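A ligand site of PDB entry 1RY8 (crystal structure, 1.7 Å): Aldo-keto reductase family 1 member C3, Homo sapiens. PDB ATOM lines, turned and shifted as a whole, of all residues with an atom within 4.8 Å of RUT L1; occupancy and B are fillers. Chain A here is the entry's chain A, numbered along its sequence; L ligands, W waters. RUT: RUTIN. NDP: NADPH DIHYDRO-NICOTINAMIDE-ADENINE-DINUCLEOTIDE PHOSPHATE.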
ATOM      1  N   TYR A  24      -2.670 -15.455   7.899  1.00  0.00           N
ATOM      2  CA  TYR A  24      -3.207 -14.727   6.764  1.00  0.00           C
ATOM      3  C   TYR A  24      -4.483 -15.291   6.177  1.00  0.00           C
ATOM      4  O   TYR A  24      -4.621 -16.498   5.959  1.00  0.00           O
ATOM      5  CB  TYR A  24      -2.174 -14.594   5.632  1.00  0.00           C
ATOM      6  CG  TYR A  24      -2.701 -13.718   4.522  1.00  0.00           C
ATOM      7  CD1 TYR A  24      -2.510 -12.340   4.536  1.00  0.00           C
ATOM      8  CD2 TYR A  24      -3.507 -14.259   3.510  1.00  0.00           C
ATOM      9  CE1 TYR A  24      -3.107 -11.515   3.584  1.00  0.00           C
ATOM     10  CE2 TYR A  24      -4.095 -13.445   2.560  1.00  0.00           C
ATOM     11  CZ  TYR A  24      -3.894 -12.072   2.604  1.00  0.00           C
ATOM     12  OH  TYR A  24      -4.485 -11.271   1.649  1.00  0.00           O
ATOM     13  N   PRO A  26      -7.494 -13.908   3.134  1.00  0.00           N
ATOM     14  CA  PRO A  26      -7.743 -12.841   2.160  1.00  0.00           C
ATOM     15  C   PRO A  26      -8.703 -11.775   2.688  1.00  0.00           C
ATOM     16  O   PRO A  26      -9.448 -12.019   3.644  1.00  0.00           O
ATOM     17  CB  PRO A  26      -8.304 -13.578   0.931  1.00  0.00           C
ATOM     18  CG  PRO A  26      -8.746 -14.895   1.451  1.00  0.00           C
ATOM     19  CD  PRO A  26      -7.875 -15.228   2.619  1.00  0.00           C
ATOM     20  N   PRO A  27      -8.696 -10.580   2.073  1.00  0.00           N
ATOM     21  CA  PRO A  27      -9.554  -9.450   2.456  1.00  0.00           C
ATOM     22  C   PRO A  27     -11.041  -9.759   2.571  1.00  0.00           C
ATOM     23  O   PRO A  27     -11.751  -9.139   3.356  1.00  0.00           O
ATOM     24  CB  PRO A  27      -9.271  -8.405   1.375  1.00  0.00           C
ATOM     25  CG  PRO A  27      -7.912  -8.749   0.880  1.00  0.00           C
ATOM     26  CD  PRO A  27      -7.834 -10.238   0.928  1.00  0.00           C
ATOM     27  N   LEU A  54       1.204  -6.308   7.016  1.00  0.00           N
ATOM     28  CA  LEU A  54       0.469  -6.447   5.758  1.00  0.00           C
ATOM     29  C   LEU A  54      -0.855  -7.226   5.869  1.00  0.00           C
ATOM     30  O   LEU A  54      -1.775  -6.976   5.095  1.00  0.00           O
ATOM     31  CB  LEU A  54       1.379  -7.110   4.718  1.00  0.00           C
ATOM     32  CG  LEU A  54       0.818  -7.362   3.314  1.00  0.00           C
ATOM     33  CD1 LEU A  54       0.761  -6.060   2.510  1.00  0.00           C
ATOM     34  CD2 LEU A  54       1.702  -8.394   2.621  1.00  0.00           C
ATOM     35  N   TYR A  55      -0.950  -8.146   6.818  1.00  0.00           N
ATOM     36  CA  TYR A  55      -2.138  -8.994   6.977  1.00  0.00           C
ATOM     37  C   TYR A  55      -3.409  -8.303   7.469  1.00  0.00           C
ATOM     38  O   TYR A  55      -4.498  -8.888   7.389  1.00  0.00           O
ATOM     39  CB  TYR A  55      -1.822 -10.159   7.928  1.00  0.00           C
ATOM     40  CG  TYR A  55      -0.650 -11.015   7.495  1.00  0.00           C
ATOM     41  CD1 TYR A  55      -0.204 -12.074   8.291  1.00  0.00           C
ATOM     42  CD2 TYR A  55       0.035 -10.755   6.306  1.00  0.00           C
ATOM     43  CE1 TYR A  55       0.892 -12.842   7.920  1.00  0.00           C
ATOM     44  CE2 TYR A  55       1.129 -11.507   5.932  1.00  0.00           C
ATOM     45  CZ  TYR A  55       1.556 -12.541   6.738  1.00  0.00           C
ATOM     46  OH  TYR A  55       2.660 -13.273   6.366  1.00  0.00           O
ATOM     47  N   TRP A  86       6.939  -4.254   6.804  1.00  0.00           N
ATOM     48  CA  TRP A  86       6.578  -4.182   5.393  1.00  0.00           C
ATOM     49  C   TRP A  86       7.616  -3.374   4.587  1.00  0.00           C
ATOM     50  O   TRP A  86       8.293  -2.488   5.109  1.00  0.00           O
ATOM     51  CB  TRP A  86       5.167  -3.594   5.215  1.00  0.00           C
ATOM     52  CG  TRP A  86       4.676  -3.698   3.800  1.00  0.00           C
ATOM     53  CD1 TRP A  86       4.151  -2.695   3.040  1.00  0.00           C
ATOM     54  CD2 TRP A  86       4.768  -4.842   2.943  1.00  0.00           C
ATOM     55  NE1 TRP A  86       3.902  -3.141   1.758  1.00  0.00           N
ATOM     56  CE2 TRP A  86       4.274  -4.459   1.670  1.00  0.00           C
ATOM     57  CE3 TRP A  86       5.220  -6.160   3.121  1.00  0.00           C
ATOM     58  CZ2 TRP A  86       4.219  -5.348   0.580  1.00  0.00           C
ATOM     59  CZ3 TRP A  86       5.165  -7.046   2.045  1.00  0.00           C
ATOM     60  CH2 TRP A  86       4.673  -6.630   0.787  1.00  0.00           C
ATOM     61  N   HIS A 117       9.989  -8.344   6.020  1.00  0.00           N
ATOM     62  CA  HIS A 117       9.048  -9.130   5.214  1.00  0.00           C
ATOM     63  C   HIS A 117       9.554  -9.559   3.835  1.00  0.00           C
ATOM     64  O   HIS A 117       9.316 -10.687   3.400  1.00  0.00           O
ATOM     65  CB  HIS A 117       7.740  -8.350   5.050  1.00  0.00           C
ATOM     66  CG  HIS A 117       6.527  -9.225   4.898  1.00  0.00           C
ATOM     67  ND1 HIS A 117       5.306  -8.891   5.442  1.00  0.00           N
ATOM     68  CD2 HIS A 117       6.348 -10.405   4.263  1.00  0.00           C
ATOM     69  CE1 HIS A 117       4.422  -9.826   5.137  1.00  0.00           C
ATOM     70  NE2 HIS A 117       5.027 -10.758   4.420  1.00  0.00           N
ATOM     71  N   MET A 120      12.567  -6.595  -1.255  1.00  0.00           N
ATOM     72  CA  MET A 120      12.181  -5.668  -2.313  1.00  0.00           C
ATOM     73  C   MET A 120      11.532  -4.371  -1.839  1.00  0.00           C
ATOM     74  O   MET A 120      10.301  -4.250  -1.791  1.00  0.00           O
ATOM     75  CB  MET A 120      11.279  -6.390  -3.314  1.00  0.00           C
ATOM     76  CG  MET A 120      12.008  -7.526  -4.026  1.00  0.00           C
ATOM     77  SD  MET A 120      11.051  -8.247  -5.358  1.00  0.00           S
ATOM     78  CE  MET A 120      10.015  -9.341  -4.448  1.00  0.00           C
ATOM     79  N   SER A 129       0.953  -0.590  -1.014  1.00  0.00           N
ATOM     80  CA  SER A 129       1.276  -0.889  -2.410  1.00  0.00           C
ATOM     81  C   SER A 129       1.242   0.380  -3.243  1.00  0.00           C
ATOM     82  O   SER A 129       0.244   0.664  -3.928  1.00  0.00           O
ATOM     83  CB  SER A 129       0.310  -1.907  -3.007  1.00  0.00           C
ATOM     84  OG  SER A 129       0.730  -2.265  -4.312  1.00  0.00           O
ATOM     85  N   ASN A 167      12.009 -14.187   2.706  1.00  0.00           N
ATOM     86  CA  ASN A 167      12.135 -14.117   1.250  1.00  0.00           C
ATOM     87  C   ASN A 167      13.516 -13.681   0.755  1.00  0.00           C
ATOM     88  O   ASN A 167      13.630 -13.107  -0.331  1.00  0.00           O
ATOM     89  CB  ASN A 167      11.062 -13.174   0.693  1.00  0.00           C
ATOM     90  CG  ASN A 167       9.659 -13.727   0.844  1.00  0.00           C
ATOM     91  OD1 ASN A 167       9.349 -14.817   0.344  1.00  0.00           O
ATOM     92  ND2 ASN A 167       8.789 -12.989   1.542  1.00  0.00           N
ATOM     93  N   GLU A 192       9.025 -19.546   1.031  1.00  0.00           N
ATOM     94  CA  GLU A 192       8.059 -20.524   0.541  1.00  0.00           C
ATOM     95  C   GLU A 192       8.810 -21.842   0.475  1.00  0.00           C
ATOM     96  O   GLU A 192       9.867 -21.945  -0.152  1.00  0.00           O
ATOM     97  CB  GLU A 192       7.563 -20.167  -0.856  1.00  0.00           C
ATOM     98  CG  GLU A 192       6.533 -21.166  -1.354  1.00  0.00           C
ATOM     99  CD  GLU A 192       5.874 -20.753  -2.652  1.00  0.00           C
ATOM    100  OE1 GLU A 192       5.416 -21.648  -3.386  1.00  0.00           O
ATOM    101  OE2 GLU A 192       5.815 -19.542  -2.930  1.00  0.00           O
ATOM    102  N   TYR A 216       6.782 -21.341   4.614  1.00  0.00           N
ATOM    103  CA  TYR A 216       5.433 -20.839   4.446  1.00  0.00           C
ATOM    104  C   TYR A 216       4.865 -21.485   3.177  1.00  0.00           C
ATOM    105  O   TYR A 216       5.629 -21.937   2.312  1.00  0.00           O
ATOM    106  CB  TYR A 216       5.378 -19.301   4.395  1.00  0.00           C
ATOM    107  CG  TYR A 216       5.916 -18.634   3.158  1.00  0.00           C
ATOM    108  CD1 TYR A 216       7.023 -17.791   3.247  1.00  0.00           C
ATOM    109  CD2 TYR A 216       5.234 -18.717   1.945  1.00  0.00           C
ATOM    110  CE1 TYR A 216       7.442 -17.031   2.152  1.00  0.00           C
ATOM    111  CE2 TYR A 216       5.645 -17.966   0.838  1.00  0.00           C
ATOM    112  CZ  TYR A 216       6.733 -17.126   0.950  1.00  0.00           C
ATOM    113  OH  TYR A 216       7.079 -16.318  -0.104  1.00  0.00           O
ATOM    114  N   GLN A 222      -2.891 -20.988  -0.413  1.00  0.00           N
ATOM    115  CA  GLN A 222      -4.343 -20.854  -0.415  1.00  0.00           C
ATOM    116  C   GLN A 222      -4.889 -20.819  -1.844  1.00  0.00           C
ATOM    117  O   GLN A 222      -6.094 -20.775  -2.062  1.00  0.00           O
ATOM    118  CB  GLN A 222      -4.740 -19.605   0.375  1.00  0.00           C
ATOM    119  CG  GLN A 222      -4.183 -19.620   1.807  1.00  0.00           C
ATOM    120  CD  GLN A 222      -4.799 -18.578   2.747  1.00  0.00           C
ATOM    121  OE1 GLN A 222      -5.975 -18.241   2.661  1.00  0.00           O
ATOM    122  NE2 GLN A 222      -3.975 -18.051   3.653  1.00  0.00           N
ATOM    123  N   ASP A 224      -5.162 -18.615  -4.426  1.00  0.00           N
ATOM    124  CA  ASP A 224      -6.125 -17.610  -4.831  1.00  0.00           C
ATOM    125  C   ASP A 224      -5.900 -17.350  -6.308  1.00  0.00           C
ATOM    126  O   ASP A 224      -4.772 -17.149  -6.748  1.00  0.00           O
ATOM    127  CB  ASP A 224      -5.897 -16.325  -4.039  1.00  0.00           C
ATOM    128  CG  ASP A 224      -7.008 -15.320  -4.254  1.00  0.00           C
ATOM    129  OD1 ASP A 224      -6.942 -14.558  -5.234  1.00  0.00           O
ATOM    130  OD2 ASP A 224      -7.956 -15.284  -3.434  1.00  0.00           O
ATOM    131  N   ARG A 226      -6.085 -14.926  -7.919  1.00  0.00           N
ATOM    132  CA  ARG A 226      -5.526 -13.607  -8.181  1.00  0.00           C
ATOM    133  C   ARG A 226      -3.998 -13.616  -8.194  1.00  0.00           C
ATOM    134  O   ARG A 226      -3.375 -12.695  -8.719  1.00  0.00           O
ATOM    135  CB  ARG A 226      -6.011 -12.598  -7.136  1.00  0.00           C
ATOM    136  CG  ARG A 226      -7.426 -12.106  -7.344  1.00  0.00           C
ATOM    137  CD  ARG A 226      -7.845 -11.159  -6.229  1.00  0.00           C
ATOM    138  NE  ARG A 226      -7.818 -11.810  -4.913  1.00  0.00           N
ATOM    139  CZ  ARG A 226      -8.336 -11.293  -3.813  1.00  0.00           C
ATOM    140  NH1 ARG A 226      -8.917 -10.098  -3.832  1.00  0.00           N
ATOM    141  NH2 ARG A 226      -8.281 -11.971  -2.665  1.00  0.00           N
ATOM    142  N   TRP A 227      -3.390 -14.647  -7.610  1.00  0.00           N
ATOM    143  CA  TRP A 227      -1.930 -14.735  -7.568  1.00  0.00           C
ATOM    144  C   TRP A 227      -1.381 -16.128  -7.824  1.00  0.00           C
ATOM    145  O   TRP A 227      -0.165 -16.297  -7.948  1.00  0.00           O
ATOM    146  CB  TRP A 227      -1.416 -14.237  -6.208  1.00  0.00           C
ATOM    147  CG  TRP A 227      -2.258 -13.143  -5.637  1.00  0.00           C
ATOM    148  CD1 TRP A 227      -3.485 -13.287  -5.048  1.00  0.00           C
ATOM    149  CD2 TRP A 227      -1.978 -11.737  -5.652  1.00  0.00           C
ATOM    150  NE1 TRP A 227      -3.980 -12.059  -4.700  1.00  0.00           N
ATOM    151  CE2 TRP A 227      -3.084 -11.089  -5.054  1.00  0.00           C
ATOM    152  CE3 TRP A 227      -0.906 -10.967  -6.118  1.00  0.00           C
ATOM    153  CZ2 TRP A 227      -3.145  -9.699  -4.907  1.00  0.00           C
ATOM    154  CZ3 TRP A 227      -0.966  -9.578  -5.971  1.00  0.00           C
ATOM    155  CH2 TRP A 227      -2.081  -8.966  -5.372  1.00  0.00           C
ATOM    156  N   PHE A 306       3.072 -18.295  -5.494  1.00  0.00           N
ATOM    157  CA  PHE A 306       2.709 -16.899  -5.690  1.00  0.00           C
ATOM    158  C   PHE A 306       3.329 -16.318  -6.953  1.00  0.00           C
ATOM    159  O   PHE A 306       4.535 -16.440  -7.188  1.00  0.00           O
ATOM    160  CB  PHE A 306       3.140 -16.063  -4.488  1.00  0.00           C
ATOM    161  CG  PHE A 306       2.361 -14.780  -4.319  1.00  0.00           C
ATOM    162  CD1 PHE A 306       2.719 -13.645  -5.038  1.00  0.00           C
ATOM    163  CD2 PHE A 306       1.293 -14.714  -3.439  1.00  0.00           C
ATOM    164  CE1 PHE A 306       2.002 -12.450  -4.874  1.00  0.00           C
ATOM    165  CE2 PHE A 306       0.578 -13.534  -3.257  1.00  0.00           C
ATOM    166  CZ  PHE A 306       0.936 -12.398  -3.975  1.00  0.00           C
ATOM    167  N   SER A 308       4.929 -13.742  -8.594  1.00  0.00           N
ATOM    168  CA  SER A 308       5.695 -12.529  -8.288  1.00  0.00           C
ATOM    169  C   SER A 308       6.291 -11.920  -9.549  1.00  0.00           C
ATOM    170  O   SER A 308       7.243 -11.134  -9.481  1.00  0.00           O
ATOM    171  CB  SER A 308       6.823 -12.881  -7.323  1.00  0.00           C
ATOM    172  OG  SER A 308       7.486 -14.060  -7.750  1.00  0.00           O
ATOM    173  N   PHE A 311       7.278  -8.252  -9.965  1.00  0.00           N
ATOM    174  CA  PHE A 311       8.463  -7.759  -9.268  1.00  0.00           C
ATOM    175  C   PHE A 311       9.766  -8.253  -9.888  1.00  0.00           C
ATOM    176  O   PHE A 311      10.853  -7.930  -9.413  1.00  0.00           O
ATOM    177  CB  PHE A 311       8.441  -8.193  -7.794  1.00  0.00           C
ATOM    178  CG  PHE A 311       7.409  -7.472  -6.981  1.00  0.00           C
ATOM    179  CD1 PHE A 311       6.256  -8.115  -6.569  1.00  0.00           C
ATOM    180  CD2 PHE A 311       7.602  -6.141  -6.624  1.00  0.00           C
ATOM    181  CE1 PHE A 311       5.285  -7.448  -5.818  1.00  0.00           C
ATOM    182  CE2 PHE A 311       6.646  -5.462  -5.876  1.00  0.00           C
ATOM    183  CZ  PHE A 311       5.490  -6.117  -5.469  1.00  0.00           C
ATOM    184  N   TYR A 319      14.356 -14.346  -6.711  1.00  0.00           N
ATOM    185  CA  TYR A 319      14.320 -15.552  -7.546  1.00  0.00           C
ATOM    186  C   TYR A 319      15.201 -15.578  -8.786  1.00  0.00           C
ATOM    187  O   TYR A 319      15.035 -16.453  -9.638  1.00  0.00           O
ATOM    188  CB  TYR A 319      12.869 -15.849  -7.926  1.00  0.00           C
ATOM    189  CG  TYR A 319      12.026 -16.333  -6.758  1.00  0.00           C
ATOM    190  CD1 TYR A 319      12.578 -17.141  -5.758  1.00  0.00           C
ATOM    191  CD2 TYR A 319      10.680 -15.989  -6.662  1.00  0.00           C
ATOM    192  CE1 TYR A 319      11.786 -17.597  -4.685  1.00  0.00           C
ATOM    193  CE2 TYR A 319       9.891 -16.435  -5.598  1.00  0.00           C
ATOM    194  CZ  TYR A 319      10.450 -17.239  -4.613  1.00  0.00           C
ATOM    195  OH  TYR A 319       9.650 -17.681  -3.578  1.00  0.00           O
HETATM  196  O1  RUT L   1      -1.633 -13.369   0.256  1.00  0.00           O
HETATM  197  C1  RUT L   1      -0.962 -12.117   0.259  1.00  0.00           C
HETATM  198  C2  RUT L   1      -1.481 -11.026  -0.426  1.00  0.00           C
HETATM  199  O2  RUT L   1      -0.827  -9.798  -0.410  1.00  0.00           O
HETATM  200  C3  RUT L   1      -2.781 -11.184  -1.185  1.00  0.00           C
HETATM  201  O3  RUT L   1      -3.299 -10.204  -1.810  1.00  0.00           O
HETATM  202  C4  RUT L   1      -4.742 -12.881  -1.800  1.00  0.00           C
HETATM  203  O4  RUT L   1      -5.355 -11.836  -2.488  1.00  0.00           O
HETATM  204  C5  RUT L   1      -5.308 -14.152  -1.699  1.00  0.00           C
HETATM  205  C6  RUT L   1      -4.567 -15.170  -0.926  1.00  0.00           C
HETATM  206  O5  RUT L   1      -5.092 -16.440  -0.812  1.00  0.00           O
HETATM  207  C7  RUT L   1      -3.311 -15.009  -0.239  1.00  0.00           C
HETATM  208  C8  RUT L   1      -2.838 -13.615  -0.414  1.00  0.00           C
HETATM  209  C9  RUT L   1      -3.441 -12.530  -1.139  1.00  0.00           C
HETATM  210  C10 RUT L   1       0.274 -12.271   1.151  1.00  0.00           C
HETATM  211  C11 RUT L   1       0.147 -13.131   2.211  1.00  0.00           C
HETATM  212  C12 RUT L   1       1.193 -13.282   3.106  1.00  0.00           C
HETATM  213  O6  RUT L   1       1.072 -14.124   4.133  1.00  0.00           O
HETATM  214  C13 RUT L   1       2.383 -12.575   2.955  1.00  0.00           C
HETATM  215  O7  RUT L   1       3.363 -12.754   3.864  1.00  0.00           O
HETATM  216  C14 RUT L   1       2.539 -11.716   1.902  1.00  0.00           C
HETATM  217  C15 RUT L   1       1.536 -11.467   0.913  1.00  0.00           C
HETATM  218  C16 RUT L   1      -0.097  -9.395  -1.623  1.00  0.00           C
HETATM  219  C17 RUT L   1      -0.374  -7.891  -1.858  1.00  0.00           C
HETATM  220  O8  RUT L   1      -1.811  -7.723  -2.041  1.00  0.00           O
HETATM  221  C18 RUT L   1       0.483  -7.470  -3.164  1.00  0.00           C
HETATM  222  O9  RUT L   1       0.247  -6.100  -3.437  1.00  0.00           O
HETATM  223  C19 RUT L   1       1.902  -7.731  -2.875  1.00  0.00           C
HETATM  224  O10 RUT L   1       2.724  -7.378  -3.978  1.00  0.00           O
HETATM  225  C20 RUT L   1       2.166  -9.277  -2.551  1.00  0.00           C
HETATM  226  C21 RUT L   1       3.622  -9.603  -2.227  1.00  0.00           C
HETATM  227  O11 RUT L   1       1.326  -9.647  -1.408  1.00  0.00           O
HETATM  228  C22 RUT L   1       4.918 -11.356  -1.177  1.00  0.00           C
HETATM  229  O12 RUT L   1       3.710 -11.037  -1.895  1.00  0.00           O
HETATM  230  C23 RUT L   1       4.907 -12.877  -0.788  1.00  0.00           C
HETATM  231  O13 RUT L   1       6.112 -13.107  -0.039  1.00  0.00           O
HETATM  232  C24 RUT L   1       4.972 -13.830  -2.018  1.00  0.00           C
HETATM  233  O14 RUT L   1       4.952 -15.212  -1.608  1.00  0.00           O
HETATM  234  C25 RUT L   1       6.260 -13.510  -2.877  1.00  0.00           C
HETATM  235  O15 RUT L   1       6.324 -14.375  -4.003  1.00  0.00           O
HETATM  236  C26 RUT L   1       6.160 -11.954  -3.271  1.00  0.00           C
HETATM  237  C27 RUT L   1       7.462 -11.568  -4.108  1.00  0.00           C
HETATM  238  O16 RUT L   1       6.099 -11.112  -2.032  1.00  0.00           O
HETATM  239  PA  NDP L   2      -0.733 -22.856   3.740  1.00  0.00           P
HETATM  240  O1A NDP L   2       0.012 -23.369   2.656  1.00  0.00           O
HETATM  241  O2A NDP L   2      -0.410 -23.058   5.201  1.00  0.00           O
HETATM  242  O5B NDP L   2      -2.231 -23.256   3.542  1.00  0.00           O
HETATM  243  C5B NDP L   2      -2.687 -24.555   3.675  1.00  0.00           C
HETATM  244  C4B NDP L   2      -4.101 -24.340   3.084  1.00  0.00           C
HETATM  245  O4B NDP L   2      -4.621 -25.687   3.222  1.00  0.00           O
HETATM  246  C3B NDP L   2      -5.009 -23.436   3.972  1.00  0.00           C
HETATM  247  O3B NDP L   2      -5.585 -22.461   3.103  1.00  0.00           O
HETATM  248  C2B NDP L   2      -6.036 -24.348   4.583  1.00  0.00           C
HETATM  249  O2B NDP L   2      -7.390 -24.040   4.290  1.00  0.00           O
HETATM  250  C1B NDP L   2      -5.714 -25.784   4.080  1.00  0.00           C
HETATM  251  N9A NDP L   2      -5.399 -26.649   5.183  1.00  0.00           N
HETATM  252  C8A NDP L   2      -4.855 -26.416   6.425  1.00  0.00           C
HETATM  253  N7A NDP L   2      -4.716 -27.502   7.167  1.00  0.00           N
HETATM  254  C5A NDP L   2      -5.196 -28.503   6.333  1.00  0.00           C
HETATM  255  C6A NDP L   2      -5.311 -29.881   6.563  1.00  0.00           C
HETATM  256  N6A NDP L   2      -4.954 -30.544   7.674  1.00  0.00           N
HETATM  257  N1A NDP L   2      -5.839 -30.655   5.538  1.00  0.00           N
HETATM  258  C2A NDP L   2      -6.241 -30.073   4.315  1.00  0.00           C
HETATM  259  N3A NDP L   2      -6.147 -28.708   4.066  1.00  0.00           N
HETATM  260  C4A NDP L   2      -5.617 -27.978   5.109  1.00  0.00           C
HETATM  261  O3  NDP L   2      -1.092 -21.352   3.492  1.00  0.00           O
HETATM  262  PN  NDP L   2      -0.287 -20.035   3.507  1.00  0.00           P
HETATM  263  O1N NDP L   2      -1.180 -18.933   3.861  1.00  0.00           O
HETATM  264  O2N NDP L   2       0.399 -19.962   2.192  1.00  0.00           O
HETATM  265  O5D NDP L   2       0.590 -20.407   4.741  1.00  0.00           O
HETATM  266  C5D NDP L   2       1.797 -19.775   5.011  1.00  0.00           C
HETATM  267  C4D NDP L   2       1.616 -18.939   6.232  1.00  0.00           C
HETATM  268  O4D NDP L   2       2.924 -18.353   6.343  1.00  0.00           O
HETATM  269  C3D NDP L   2       0.613 -17.707   6.133  1.00  0.00           C
HETATM  270  O3D NDP L   2      -0.662 -17.878   6.765  1.00  0.00           O
HETATM  271  C2D NDP L   2       1.431 -16.567   6.714  1.00  0.00           C
HETATM  272  O2D NDP L   2       1.321 -16.496   8.125  1.00  0.00           O
HETATM  273  C1D NDP L   2       2.822 -16.908   6.327  1.00  0.00           C
HETATM  274  N1N NDP L   2       3.304 -16.423   4.964  1.00  0.00           N
HETATM  275  C2N NDP L   2       4.449 -15.616   4.886  1.00  0.00           C
HETATM  276  C3N NDP L   2       4.849 -15.161   3.647  1.00  0.00           C
HETATM  277  C7N NDP L   2       6.075 -14.261   3.577  1.00  0.00           C
HETATM  278  O7N NDP L   2       6.368 -13.833   2.490  1.00  0.00           O
HETATM  279  N7N NDP L   2       6.744 -13.947   4.655  1.00  0.00           N
HETATM  280  C4N NDP L   2       4.131 -15.502   2.410  1.00  0.00           C
HETATM  281  C5N NDP L   2       2.985 -16.333   2.514  1.00  0.00           C
HETATM  282  C6N NDP L   2       2.552 -16.804   3.779  1.00  0.00           C
HETATM  283  P2B NDP L   2      -8.481 -23.908   5.468  1.00  0.00           P
HETATM  284  O1X NDP L   2      -8.276 -22.518   6.072  1.00  0.00           O
HETATM  285  O2X NDP L   2      -9.754 -24.050   4.712  1.00  0.00           O
HETATM  286  O3X NDP L   2      -8.175 -25.005   6.469  1.00  0.00           O
HETATM  287  O   HOH W   1       2.194 -16.110  -0.708  1.00  0.00           O
HETATM  288  O   HOH W   2      -2.894 -17.449  -2.974  1.00  0.00           O
HETATM  289  O   HOH W   3      -4.806  -7.283  -2.020  1.00  0.00           O
HETATM  290  O   HOH W   4       7.568  -8.711  -1.898  1.00  0.00           O
HETATM  291  O   HOH W   5      -7.959 -17.021  -1.083  1.00  0.00           O
HETATM  292  O   HOH W   6      -0.734 -16.382   2.746  1.00  0.00           O
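An oxygen (O4) of RUT L1 lies within hydrogen-bond range of the indole nitrogen (NE1) of Trp 227, 2.6 Å away. OH of Tyr 55 sits at hydrogen-bond distance from O7 of RUT L1, 2.7 Å away. NE2 of His 117 lies within hydrogen-bond range of O7 of RUT L1, at 2.7 Å. O14 of RUT L1 is in hydrogen-bond range of OH of Tyr 216, 2.8 Å away. NH2 of Arg 226 is in hydrogen-bond range of O4 of RUT L1, at 2.9 Å. The side-chain amide nitrogen (ND2) of Asn 167 sits at hydrogen-bond distance from an oxygen (O13) of RUT L1, 3.1 Å away. O7N of NDP L2 lies within hydrogen-bond range of ND2 of Asn 167, 2.7 Å away. N of Tyr 24 is in hydrogen-bond range of O3D of NDP L2, at 3.3 Å. NE2 of Gln 222 sits at hydrogen-bond distance from O1N of NDP L2, 2.9 Å away.
Merely in contact with RUT L1: Phe 311, Tyr 24, Asp 224, Gln 222, Met 120, Leu 54, Phe 306, Ser 308 and Ser 129. Within 4 Å of RUT L1: Tyr 24, Leu 54, Tyr 55, His 117, Met 120, Ser 129, Asn 167, Tyr 216, Gln 222, Asp 224, Arg 226, Trp 227, Phe 306, Ser 308 and Phe 311. The nearest printed residue that does not touch RUT L1 is Pro 26 (4.03 Å).
Water W5 bridges the side-chain carboxylate (OD2) of Asp 224 and an oxygen (O5) of RUT L1. Water W6 bridges O1N of NDP L2 and O6 of RUT L1. Water W2 bridges N of Asp 224 (2.9 Å) and O5 of RUT L1 (3.2 Å).
An oxygen (O13) of RUT L1 lies within hydrogen-bond range of an oxygen (O7N) of NDP L2 (2.6 Å).
The backbone carbonyl oxygen (O) of His 117 lies within hydrogen-bond range of the side-chain amide nitrogen (ND2) of Asn 167 (3.0 Å). OH of Tyr 216 is in hydrogen-bond range of OD1 of Asn 167 (2.8 Å). NE of Arg 226 is in salt-bridge range of OD1 of Asp 224 (2.9 Å). The backbone carbonyl oxygen (O) of Tyr 24 sits at hydrogen-bond distance from the side-chain amide nitrogen (NE2) of Gln 222 (2.9 Å).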
